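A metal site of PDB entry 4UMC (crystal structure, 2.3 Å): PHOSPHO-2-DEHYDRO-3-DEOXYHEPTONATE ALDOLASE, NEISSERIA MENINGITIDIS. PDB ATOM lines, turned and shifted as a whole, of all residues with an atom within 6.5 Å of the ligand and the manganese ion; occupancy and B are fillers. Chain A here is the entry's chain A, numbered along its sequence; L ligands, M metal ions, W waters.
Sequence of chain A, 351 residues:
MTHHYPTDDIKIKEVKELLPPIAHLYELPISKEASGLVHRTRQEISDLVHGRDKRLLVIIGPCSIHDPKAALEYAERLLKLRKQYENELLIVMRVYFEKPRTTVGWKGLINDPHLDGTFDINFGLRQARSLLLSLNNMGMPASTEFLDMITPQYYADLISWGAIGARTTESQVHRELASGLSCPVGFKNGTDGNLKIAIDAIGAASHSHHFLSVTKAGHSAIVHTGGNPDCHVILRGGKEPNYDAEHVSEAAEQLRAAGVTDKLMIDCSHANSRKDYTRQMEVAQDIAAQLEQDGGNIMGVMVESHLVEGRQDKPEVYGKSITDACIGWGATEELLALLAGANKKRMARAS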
ATOM      1  N   PRO A  62     -31.766  10.648  17.126  1.00  0.00           N
ATOM      2  CA  PRO A  62     -31.078  11.810  17.653  1.00  0.00           C
ATOM      3  C   PRO A  62     -30.511  11.663  19.050  1.00  0.00           C
ATOM      4  O   PRO A  62     -30.957  10.843  19.851  1.00  0.00           O
ATOM      5  CB  PRO A  62     -32.158  12.881  17.675  1.00  0.00           C
ATOM      6  CG  PRO A  62     -33.108  12.455  16.604  1.00  0.00           C
ATOM      7  CD  PRO A  62     -33.130  10.949  16.688  1.00  0.00           C
ATOM      8  N   CYS A  63     -29.500  12.452  19.345  1.00  0.00           N
ATOM      9  CA  CYS A  63     -28.949  12.479  20.695  1.00  0.00           C
ATOM     10  C   CYS A  63     -30.091  12.963  21.571  1.00  0.00           C
ATOM     11  O   CYS A  63     -30.355  12.356  22.604  1.00  0.00           O
ATOM     12  CB  CYS A  63     -27.742  13.400  20.780  1.00  0.00           C
ATOM     13  SG  CYS A  63     -27.183  13.780  22.451  1.00  0.00           S
ATOM     14  N   SER A  64     -30.784  14.028  21.137  1.00  0.00           N
ATOM     15  CA  SER A  64     -31.917  14.571  21.859  1.00  0.00           C
ATOM     16  C   SER A  64     -32.978  15.028  20.906  1.00  0.00           C
ATOM     17  O   SER A  64     -32.659  15.484  19.836  1.00  0.00           O
ATOM     18  CB  SER A  64     -31.498  15.787  22.678  1.00  0.00           C
ATOM     19  OG  SER A  64     -30.867  16.763  21.861  1.00  0.00           O
ATOM     20  N   ARG A  94     -34.348   6.280  19.012  1.00  0.00           N
ATOM     21  CA  ARG A  94     -33.956   7.103  20.136  1.00  0.00           C
ATOM     22  C   ARG A  94     -34.881   8.294  20.178  1.00  0.00           C
ATOM     23  O   ARG A  94     -34.845   9.134  19.261  1.00  0.00           O
ATOM     24  CB  ARG A  94     -32.539   7.654  20.010  1.00  0.00           C
ATOM     25  CG  ARG A  94     -31.435   6.653  20.219  1.00  0.00           C
ATOM     26  CD  ARG A  94     -30.070   7.296  20.065  1.00  0.00           C
ATOM     27  NE  ARG A  94     -29.982   8.490  20.925  1.00  0.00           N
ATOM     28  CZ  ARG A  94     -29.227   8.626  22.015  1.00  0.00           C
ATOM     29  NH1 ARG A  94     -28.408   7.676  22.435  1.00  0.00           N
ATOM     30  NH2 ARG A  94     -29.267   9.774  22.665  1.00  0.00           N
ATOM     31  N   TYR A  96     -34.997  10.723  22.954  1.00  0.00           N
ATOM     32  CA  TYR A  96     -34.484  11.175  24.267  1.00  0.00           C
ATOM     33  C   TYR A  96     -35.013  12.545  24.683  1.00  0.00           C
ATOM     34  O   TYR A  96     -34.744  13.556  24.027  1.00  0.00           O
ATOM     35  CB  TYR A  96     -32.972  11.171  24.273  1.00  0.00           C
ATOM     36  CG  TYR A  96     -32.330   9.802  24.475  1.00  0.00           C
ATOM     37  CD1 TYR A  96     -32.786   8.657  23.791  1.00  0.00           C
ATOM     38  CD2 TYR A  96     -31.248   9.641  25.335  1.00  0.00           C
ATOM     39  CE1 TYR A  96     -32.160   7.412  23.946  1.00  0.00           C
ATOM     40  CE2 TYR A  96     -30.627   8.404  25.493  1.00  0.00           C
ATOM     41  CZ  TYR A  96     -31.082   7.304  24.795  1.00  0.00           C
ATOM     42  OH  TYR A  96     -30.443   6.114  25.021  1.00  0.00           O
ATOM     43  N   LYS A  99     -31.683  15.028  29.223  1.00  0.00           N
ATOM     44  CA  LYS A  99     -30.235  15.041  28.942  1.00  0.00           C
ATOM     45  C   LYS A  99     -29.413  15.395  30.221  1.00  0.00           C
ATOM     46  O   LYS A  99     -29.671  16.411  30.872  1.00  0.00           O
ATOM     47  CB  LYS A  99     -29.930  16.055  27.830  1.00  0.00           C
ATOM     48  CG  LYS A  99     -30.655  15.831  26.518  1.00  0.00           C
ATOM     49  CD  LYS A  99     -30.510  14.400  26.004  1.00  0.00           C
ATOM     50  CE  LYS A  99     -29.085  14.060  25.678  1.00  0.00           C
ATOM     51  NZ  LYS A  99     -28.979  12.685  25.123  1.00  0.00           N
ATOM     52  N   PRO A 100     -28.410  14.580  30.555  1.00  0.00           N
ATOM     53  CA  PRO A 100     -27.528  14.861  31.679  1.00  0.00           C
ATOM     54  C   PRO A 100     -26.355  15.674  31.248  1.00  0.00           C
ATOM     55  O   PRO A 100     -25.583  15.260  30.380  1.00  0.00           O
ATOM     56  CB  PRO A 100     -27.067  13.478  32.106  1.00  0.00           C
ATOM     57  CG  PRO A 100     -27.087  12.670  30.871  1.00  0.00           C
ATOM     58  CD  PRO A 100     -28.213  13.212  30.033  1.00  0.00           C
ATOM     59  N   GLU A 145     -33.704   7.809  27.571  1.00  0.00           N
ATOM     60  CA  GLU A 145     -32.958   7.668  28.817  1.00  0.00           C
ATOM     61  C   GLU A 145     -33.859   8.106  29.932  1.00  0.00           C
ATOM     62  O   GLU A 145     -34.467   9.165  29.855  1.00  0.00           O
ATOM     63  CB  GLU A 145     -31.669   8.520  28.860  1.00  0.00           C
ATOM     64  CG  GLU A 145     -31.027   8.469  30.237  1.00  0.00           C
ATOM     65  CD  GLU A 145     -29.748   9.242  30.420  1.00  0.00           C
ATOM     66  OE1 GLU A 145     -29.094   9.577  29.409  1.00  0.00           O
ATOM     67  OE2 GLU A 145     -29.398   9.485  31.612  1.00  0.00           O
ATOM     68  N   ILE A 164     -30.305   3.787  31.263  1.00  0.00           N
ATOM     69  CA  ILE A 164     -29.801   4.520  32.414  1.00  0.00           C
ATOM     70  C   ILE A 164     -28.403   4.933  32.076  1.00  0.00           C
ATOM     71  O   ILE A 164     -27.542   4.092  31.744  1.00  0.00           O
ATOM     72  CB  ILE A 164     -29.787   3.683  33.670  1.00  0.00           C
ATOM     73  CG1 ILE A 164     -31.212   3.229  34.033  1.00  0.00           C
ATOM     74  CG2 ILE A 164     -29.152   4.479  34.818  1.00  0.00           C
ATOM     75  CD1 ILE A 164     -32.147   4.328  34.451  1.00  0.00           C
ATOM     76  N   GLY A 165     -28.184   6.234  32.119  1.00  0.00           N
ATOM     77  CA  GLY A 165     -26.945   6.815  31.589  1.00  0.00           C
ATOM     78  C   GLY A 165     -25.690   6.487  32.365  1.00  0.00           C
ATOM     79  O   GLY A 165     -25.734   6.058  33.501  1.00  0.00           O
ATOM     80  N   ALA A 166     -24.564   6.768  31.734  1.00  0.00           N
ATOM     81  CA  ALA A 166     -23.264   6.485  32.296  1.00  0.00           C
ATOM     82  C   ALA A 166     -23.094   7.184  33.662  1.00  0.00           C
ATOM     83  O   ALA A 166     -22.448   6.663  34.538  1.00  0.00           O
ATOM     84  CB  ALA A 166     -22.164   6.924  31.347  1.00  0.00           C
ATOM     85  N   ARG A 167     -23.691   8.355  33.785  1.00  0.00           N
ATOM     86  CA  ARG A 167     -23.559   9.214  34.956  1.00  0.00           C
ATOM     87  C   ARG A 167     -24.487   8.868  36.075  1.00  0.00           C
ATOM     88  O   ARG A 167     -24.432   9.495  37.135  1.00  0.00           O
ATOM     89  CB  ARG A 167     -23.812  10.670  34.563  1.00  0.00           C
ATOM     90  CG  ARG A 167     -22.759  11.184  33.602  1.00  0.00           C
ATOM     91  CD  ARG A 167     -23.064  12.575  33.043  1.00  0.00           C
ATOM     92  NE  ARG A 167     -22.122  12.864  31.962  1.00  0.00           N
ATOM     93  CZ  ARG A 167     -22.161  12.334  30.731  1.00  0.00           C
ATOM     94  NH1 ARG A 167     -23.104  11.468  30.364  1.00  0.00           N
ATOM     95  NH2 ARG A 167     -21.236  12.673  29.860  1.00  0.00           N
ATOM     96  N   LYS A 188     -25.442   1.720  31.224  1.00  0.00           N
ATOM     97  CA  LYS A 188     -24.200   2.081  30.586  1.00  0.00           C
ATOM     98  C   LYS A 188     -23.052   2.034  31.552  1.00  0.00           C
ATOM     99  O   LYS A 188     -23.221   2.323  32.694  1.00  0.00           O
ATOM    100  CB  LYS A 188     -24.298   3.479  30.061  1.00  0.00           C
ATOM    101  CG  LYS A 188     -25.301   3.570  28.921  1.00  0.00           C
ATOM    102  CD  LYS A 188     -25.185   4.899  28.207  1.00  0.00           C
ATOM    103  CE  LYS A 188     -25.151   4.683  26.716  1.00  0.00           C
ATOM    104  NZ  LYS A 188     -25.011   6.000  26.067  1.00  0.00           N
ATOM    105  N   ASN A 189     -21.880   1.643  31.070  1.00  0.00           N
ATOM    106  CA  ASN A 189     -20.693   1.731  31.873  1.00  0.00           C
ATOM    107  C   ASN A 189     -20.393   3.178  32.205  1.00  0.00           C
ATOM    108  O   ASN A 189     -20.909   4.083  31.558  1.00  0.00           O
ATOM    109  CB  ASN A 189     -19.499   1.010  31.214  1.00  0.00           C
ATOM    110  CG  ASN A 189     -19.008   1.682  29.937  1.00  0.00           C
ATOM    111  OD1 ASN A 189     -19.064   1.086  28.863  1.00  0.00           O
ATOM    112  ND2 ASN A 189     -18.443   2.866  30.048  1.00  0.00           N
ATOM    113  N   THR A 191     -18.432   6.888  33.053  1.00  0.00           N
ATOM    114  CA  THR A 191     -17.835   7.799  32.095  1.00  0.00           C
ATOM    115  C   THR A 191     -16.334   7.598  31.950  1.00  0.00           C
ATOM    116  O   THR A 191     -15.777   7.974  30.929  1.00  0.00           O
ATOM    117  CB  THR A 191     -18.145   9.270  32.407  1.00  0.00           C
ATOM    118  OG1 THR A 191     -17.778   9.537  33.749  1.00  0.00           O
ATOM    119  CG2 THR A 191     -19.604   9.559  32.239  1.00  0.00           C
ATOM    120  N   ARG A 236     -20.145   1.845  26.287  1.00  0.00           N
ATOM    121  CA  ARG A 236     -20.134   3.175  25.676  1.00  0.00           C
ATOM    122  C   ARG A 236     -18.788   3.910  25.633  1.00  0.00           C
ATOM    123  O   ARG A 236     -18.736   5.104  25.371  1.00  0.00           O
ATOM    124  CB  ARG A 236     -21.211   4.072  26.314  1.00  0.00           C
ATOM    125  CG  ARG A 236     -21.114   4.188  27.825  1.00  0.00           C
ATOM    126  CD  ARG A 236     -20.071   5.219  28.229  1.00  0.00           C
ATOM    127  NE  ARG A 236     -20.568   6.583  28.146  1.00  0.00           N
ATOM    128  CZ  ARG A 236     -19.806   7.673  28.242  1.00  0.00           C
ATOM    129  NH1 ARG A 236     -18.504   7.544  28.422  1.00  0.00           N
ATOM    130  NH2 ARG A 236     -20.347   8.874  28.145  1.00  0.00           N
ATOM    131  N   ASP A 267     -22.546   0.831  22.232  1.00  0.00           N
ATOM    132  CA  ASP A 267     -22.841   2.167  21.756  1.00  0.00           C
ATOM    133  C   ASP A 267     -21.735   2.587  20.769  1.00  0.00           C
ATOM    134  O   ASP A 267     -20.575   2.595  21.123  1.00  0.00           O
ATOM    135  CB  ASP A 267     -22.930   3.133  22.931  1.00  0.00           C
ATOM    136  CG  ASP A 267     -23.356   4.549  22.540  1.00  0.00           C
ATOM    137  OD1 ASP A 267     -23.634   4.848  21.357  1.00  0.00           O
ATOM    138  OD2 ASP A 267     -23.438   5.383  23.471  1.00  0.00           O
ATOM    139  N   SER A 269     -21.583   5.563  19.548  1.00  0.00           N
ATOM    140  CA  SER A 269     -21.370   6.974  19.830  1.00  0.00           C
ATOM    141  C   SER A 269     -20.612   7.251  21.128  1.00  0.00           C
ATOM    142  O   SER A 269     -20.116   6.342  21.783  1.00  0.00           O
ATOM    143  CB  SER A 269     -22.697   7.741  19.821  1.00  0.00           C
ATOM    144  OG  SER A 269     -22.522   9.035  19.306  1.00  0.00           O
ATOM    145  N   HIS A 270     -20.541   8.537  21.482  1.00  0.00           N
ATOM    146  CA  HIS A 270     -19.978   8.962  22.760  1.00  0.00           C
ATOM    147  C   HIS A 270     -18.514   8.570  22.940  1.00  0.00           C
ATOM    148  O   HIS A 270     -17.687   8.875  22.087  1.00  0.00           O
ATOM    149  CB  HIS A 270     -20.858   8.479  23.913  1.00  0.00           C
ATOM    150  CG  HIS A 270     -22.280   8.936  23.795  1.00  0.00           C
ATOM    151  ND1 HIS A 270     -23.308   8.085  23.440  1.00  0.00           N
ATOM    152  CD2 HIS A 270     -22.847  10.147  23.958  1.00  0.00           C
ATOM    153  CE1 HIS A 270     -24.451   8.754  23.411  1.00  0.00           C
ATOM    154  NE2 HIS A 270     -24.187  10.008  23.721  1.00  0.00           N
ATOM    155  N   ALA A 271     -18.173   7.933  24.058  1.00  0.00           N
ATOM    156  CA  ALA A 271     -16.758   7.688  24.294  1.00  0.00           C
ATOM    157  C   ALA A 271     -16.197   6.626  23.360  1.00  0.00           C
ATOM    158  O   ALA A 271     -14.978   6.513  23.227  1.00  0.00           O
ATOM    159  CB  ALA A 271     -16.503   7.322  25.776  1.00  0.00           C
ATOM    160  N   MET A 302     -26.176   0.886  19.454  1.00  0.00           N
ATOM    161  CA  MET A 302     -26.757   2.216  19.677  1.00  0.00           C
ATOM    162  C   MET A 302     -26.054   3.153  18.707  1.00  0.00           C
ATOM    163  O   MET A 302     -24.831   3.128  18.610  1.00  0.00           O
ATOM    164  CB  MET A 302     -26.513   2.624  21.123  1.00  0.00           C
ATOM    165  CG  MET A 302     -26.985   4.005  21.543  1.00  0.00           C
ATOM    166  SD  MET A 302     -27.167   4.225  23.359  1.00  0.00           S
ATOM    167  CE  MET A 302     -27.645   2.590  23.868  1.00  0.00           C
ATOM    168  N   GLU A 304     -26.129   7.338  17.167  1.00  0.00           N
ATOM    169  CA  GLU A 304     -26.652   8.711  17.171  1.00  0.00           C
ATOM    170  C   GLU A 304     -26.753   9.240  15.728  1.00  0.00           C
ATOM    171  O   GLU A 304     -25.748   9.498  15.051  1.00  0.00           O
ATOM    172  CB  GLU A 304     -25.806   9.612  18.077  1.00  0.00           C
ATOM    173  CG  GLU A 304     -26.146   9.423  19.562  1.00  0.00           C
ATOM    174  CD  GLU A 304     -25.412  10.368  20.517  1.00  0.00           C
ATOM    175  OE1 GLU A 304     -24.205  10.655  20.323  1.00  0.00           O
ATOM    176  OE2 GLU A 304     -26.068  10.782  21.506  1.00  0.00           O
ATOM    177  N   THR A 323     -27.535  18.979  20.618  1.00  0.00           N
ATOM    178  CA  THR A 323     -26.700  18.252  21.582  1.00  0.00           C
ATOM    179  C   THR A 323     -25.573  17.556  20.823  1.00  0.00           C
ATOM    180  O   THR A 323     -24.957  18.149  19.951  1.00  0.00           O
ATOM    181  CB  THR A 323     -27.507  17.269  22.441  1.00  0.00           C
ATOM    182  OG1 THR A 323     -28.405  16.513  21.624  1.00  0.00           O
ATOM    183  CG2 THR A 323     -28.308  18.023  23.481  1.00  0.00           C
ATOM    184  N   ASP A 324     -25.270  16.306  21.171  1.00  0.00           N
ATOM    185  CA  ASP A 324     -24.130  15.634  20.552  1.00  0.00           C
ATOM    186  C   ASP A 324     -24.339  15.525  19.030  1.00  0.00           C
ATOM    187  O   ASP A 324     -25.462  15.361  18.535  1.00  0.00           O
ATOM    188  CB  ASP A 324     -23.901  14.217  21.145  1.00  0.00           C
ATOM    189  CG  ASP A 324     -23.686  14.232  22.658  1.00  0.00           C
ATOM    190  OD1 ASP A 324     -23.077  15.198  23.134  1.00  0.00           O
ATOM    191  OD2 ASP A 324     -24.086  13.254  23.304  1.00  0.00           O
HETATM  192  C1  LIG L   1     -26.863  10.199  25.365  1.00  0.00           C
HETATM  193  O1  LIG L   1     -27.164   9.080  24.889  1.00  0.00           O
HETATM  194  O2  LIG L   1     -27.013  11.311  24.773  1.00  0.00           O
HETATM  195  C2  LIG L   1     -26.180  10.158  26.783  1.00  0.00           C
HETATM  196  C3  LIG L   1     -25.694  11.533  27.304  1.00  0.00           C
HETATM  197  O3  LIG L   1     -25.074   9.199  26.750  1.00  0.00           O
HETATM  198  P1  LIG L   1     -24.123   8.722  28.054  1.00  0.00           P
HETATM  199  O4  LIG L   1     -23.312   7.436  27.582  1.00  0.00           O
HETATM  200  O5  LIG L   1     -23.017   9.925  28.185  1.00  0.00           O
HETATM  201  O6  LIG L   1     -24.897   8.366  29.255  1.00  0.00           O
HETATM  202 MN    MN M   1     -25.513  11.872  23.181  1.00  0.00          MN
HETATM  203  O   HOH W   1     -25.070   9.734  31.531  1.00  0.00           O
HETATM  204  O   HOH W   2     -27.720   7.504  28.552  1.00  0.00           O
HETATM  205  O   HOH W   3     -26.177  14.521  27.562  1.00  0.00           O
HETATM  206  O   HOH W   4     -27.873   6.552  26.289  1.00  0.00           O
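The side-chain amino group of Lys 99 sits close to an oxygen (O2) of the ligand (2.4 Å).
The guanidinium group (NH1) of Arg 167 is in salt-bridge range of an oxygen (O5) of the ligand (2.7 Å).
NZ of Lys 188 is in salt-bridge range of O4 of the ligand (2.7 Å).
O5 of the ligand lies within salt-bridge range of NH2 of Arg 236 (2.9 Å).
N of Ala 166 sits at hydrogen-bond distance from O6 of the ligand.
The guanidinium group (NH1) of Arg 94 lies within salt-bridge range of an oxygen (O1) of the ligand.
The guanidinium group (NH2) of Arg 94 sits close to the side-chain carboxylate (OE2) of Glu 304, 3.5 Å away.
The side-chain carboxylate (OE1) of Glu 304 is in hydrogen-bond range of the side-chain hydroxyl (OG) of Ser 269, at 2.5 Å.
ND1 of His 270 is in hydrogen-bond range of OD2 of Asp 267 (2.7 Å).
O of Cys 63 lies within hydrogen-bond range of NH2 of Arg 94 (2.8 Å).
The side-chain amino group of Lys 188 lies within salt-bridge range of the side-chain carboxylate of Asp 267.
OD1 of Asn 189 lies within hydrogen-bond range of N of Arg 236 (2.9 Å).
The backbone carbonyl oxygen (O) of Arg 236 lies within hydrogen-bond range of the backbone NH (N) of Ala 271 (3.2 Å).
The guanidinium group of Arg 94 sits at hydrogen-bond distance from the backbone carbonyl oxygen of Pro 62, 2.8 Å away.
Merely in contact with the ligand: Tyr 96 (3.6 Å), Pro 100 (3.99 Å), Glu 145 (3.97 Å) and Gly 165 (3.5 Å).
14 residues have an atom within 4 Å of the ligand: Cys 63, Arg 94, Tyr 96, Lys 99, Pro 100, Glu 145, Gly 165, Ala 166, Arg 167, Lys 188, Arg 236, His 270, Glu 304 and Asp 324.
The nearest printed residue that does not touch the ligand is Asp 267 (4.6 Å).
Within 4 Å of the manganese ion: Cys 63, His 270, Glu 304 and Asp 324.
The nearest printed residue that does not touch the manganese ion is Lys 99 (4.1 Å).
The manganese ion is bound by OD2 of Asp 324 (2.0 Å), OE2 of Glu 304 (2.1 Å), O2 of the ligand (2.3 Å), NE2 of His 270 (2.4 Å) and SG of Cys 63 (2.6 Å).
Water W1 lies within hydrogen-bond range of an oxygen (O6) of the ligand (2.7 Å), the guanidinium group of Arg 167 (2.9 Å) and the backbone NH of Ala 166 (3.0 Å).
Water W4 lies within hydrogen-bond range of OH of Tyr 96 (2.9 Å), NZ of Lys 188 (2.9 Å) and O1 of the ligand (3.0 Å).
Water W2 bridges OE1 of Glu 145 (2.6 Å) and O6 of the ligand (3.0 Å).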
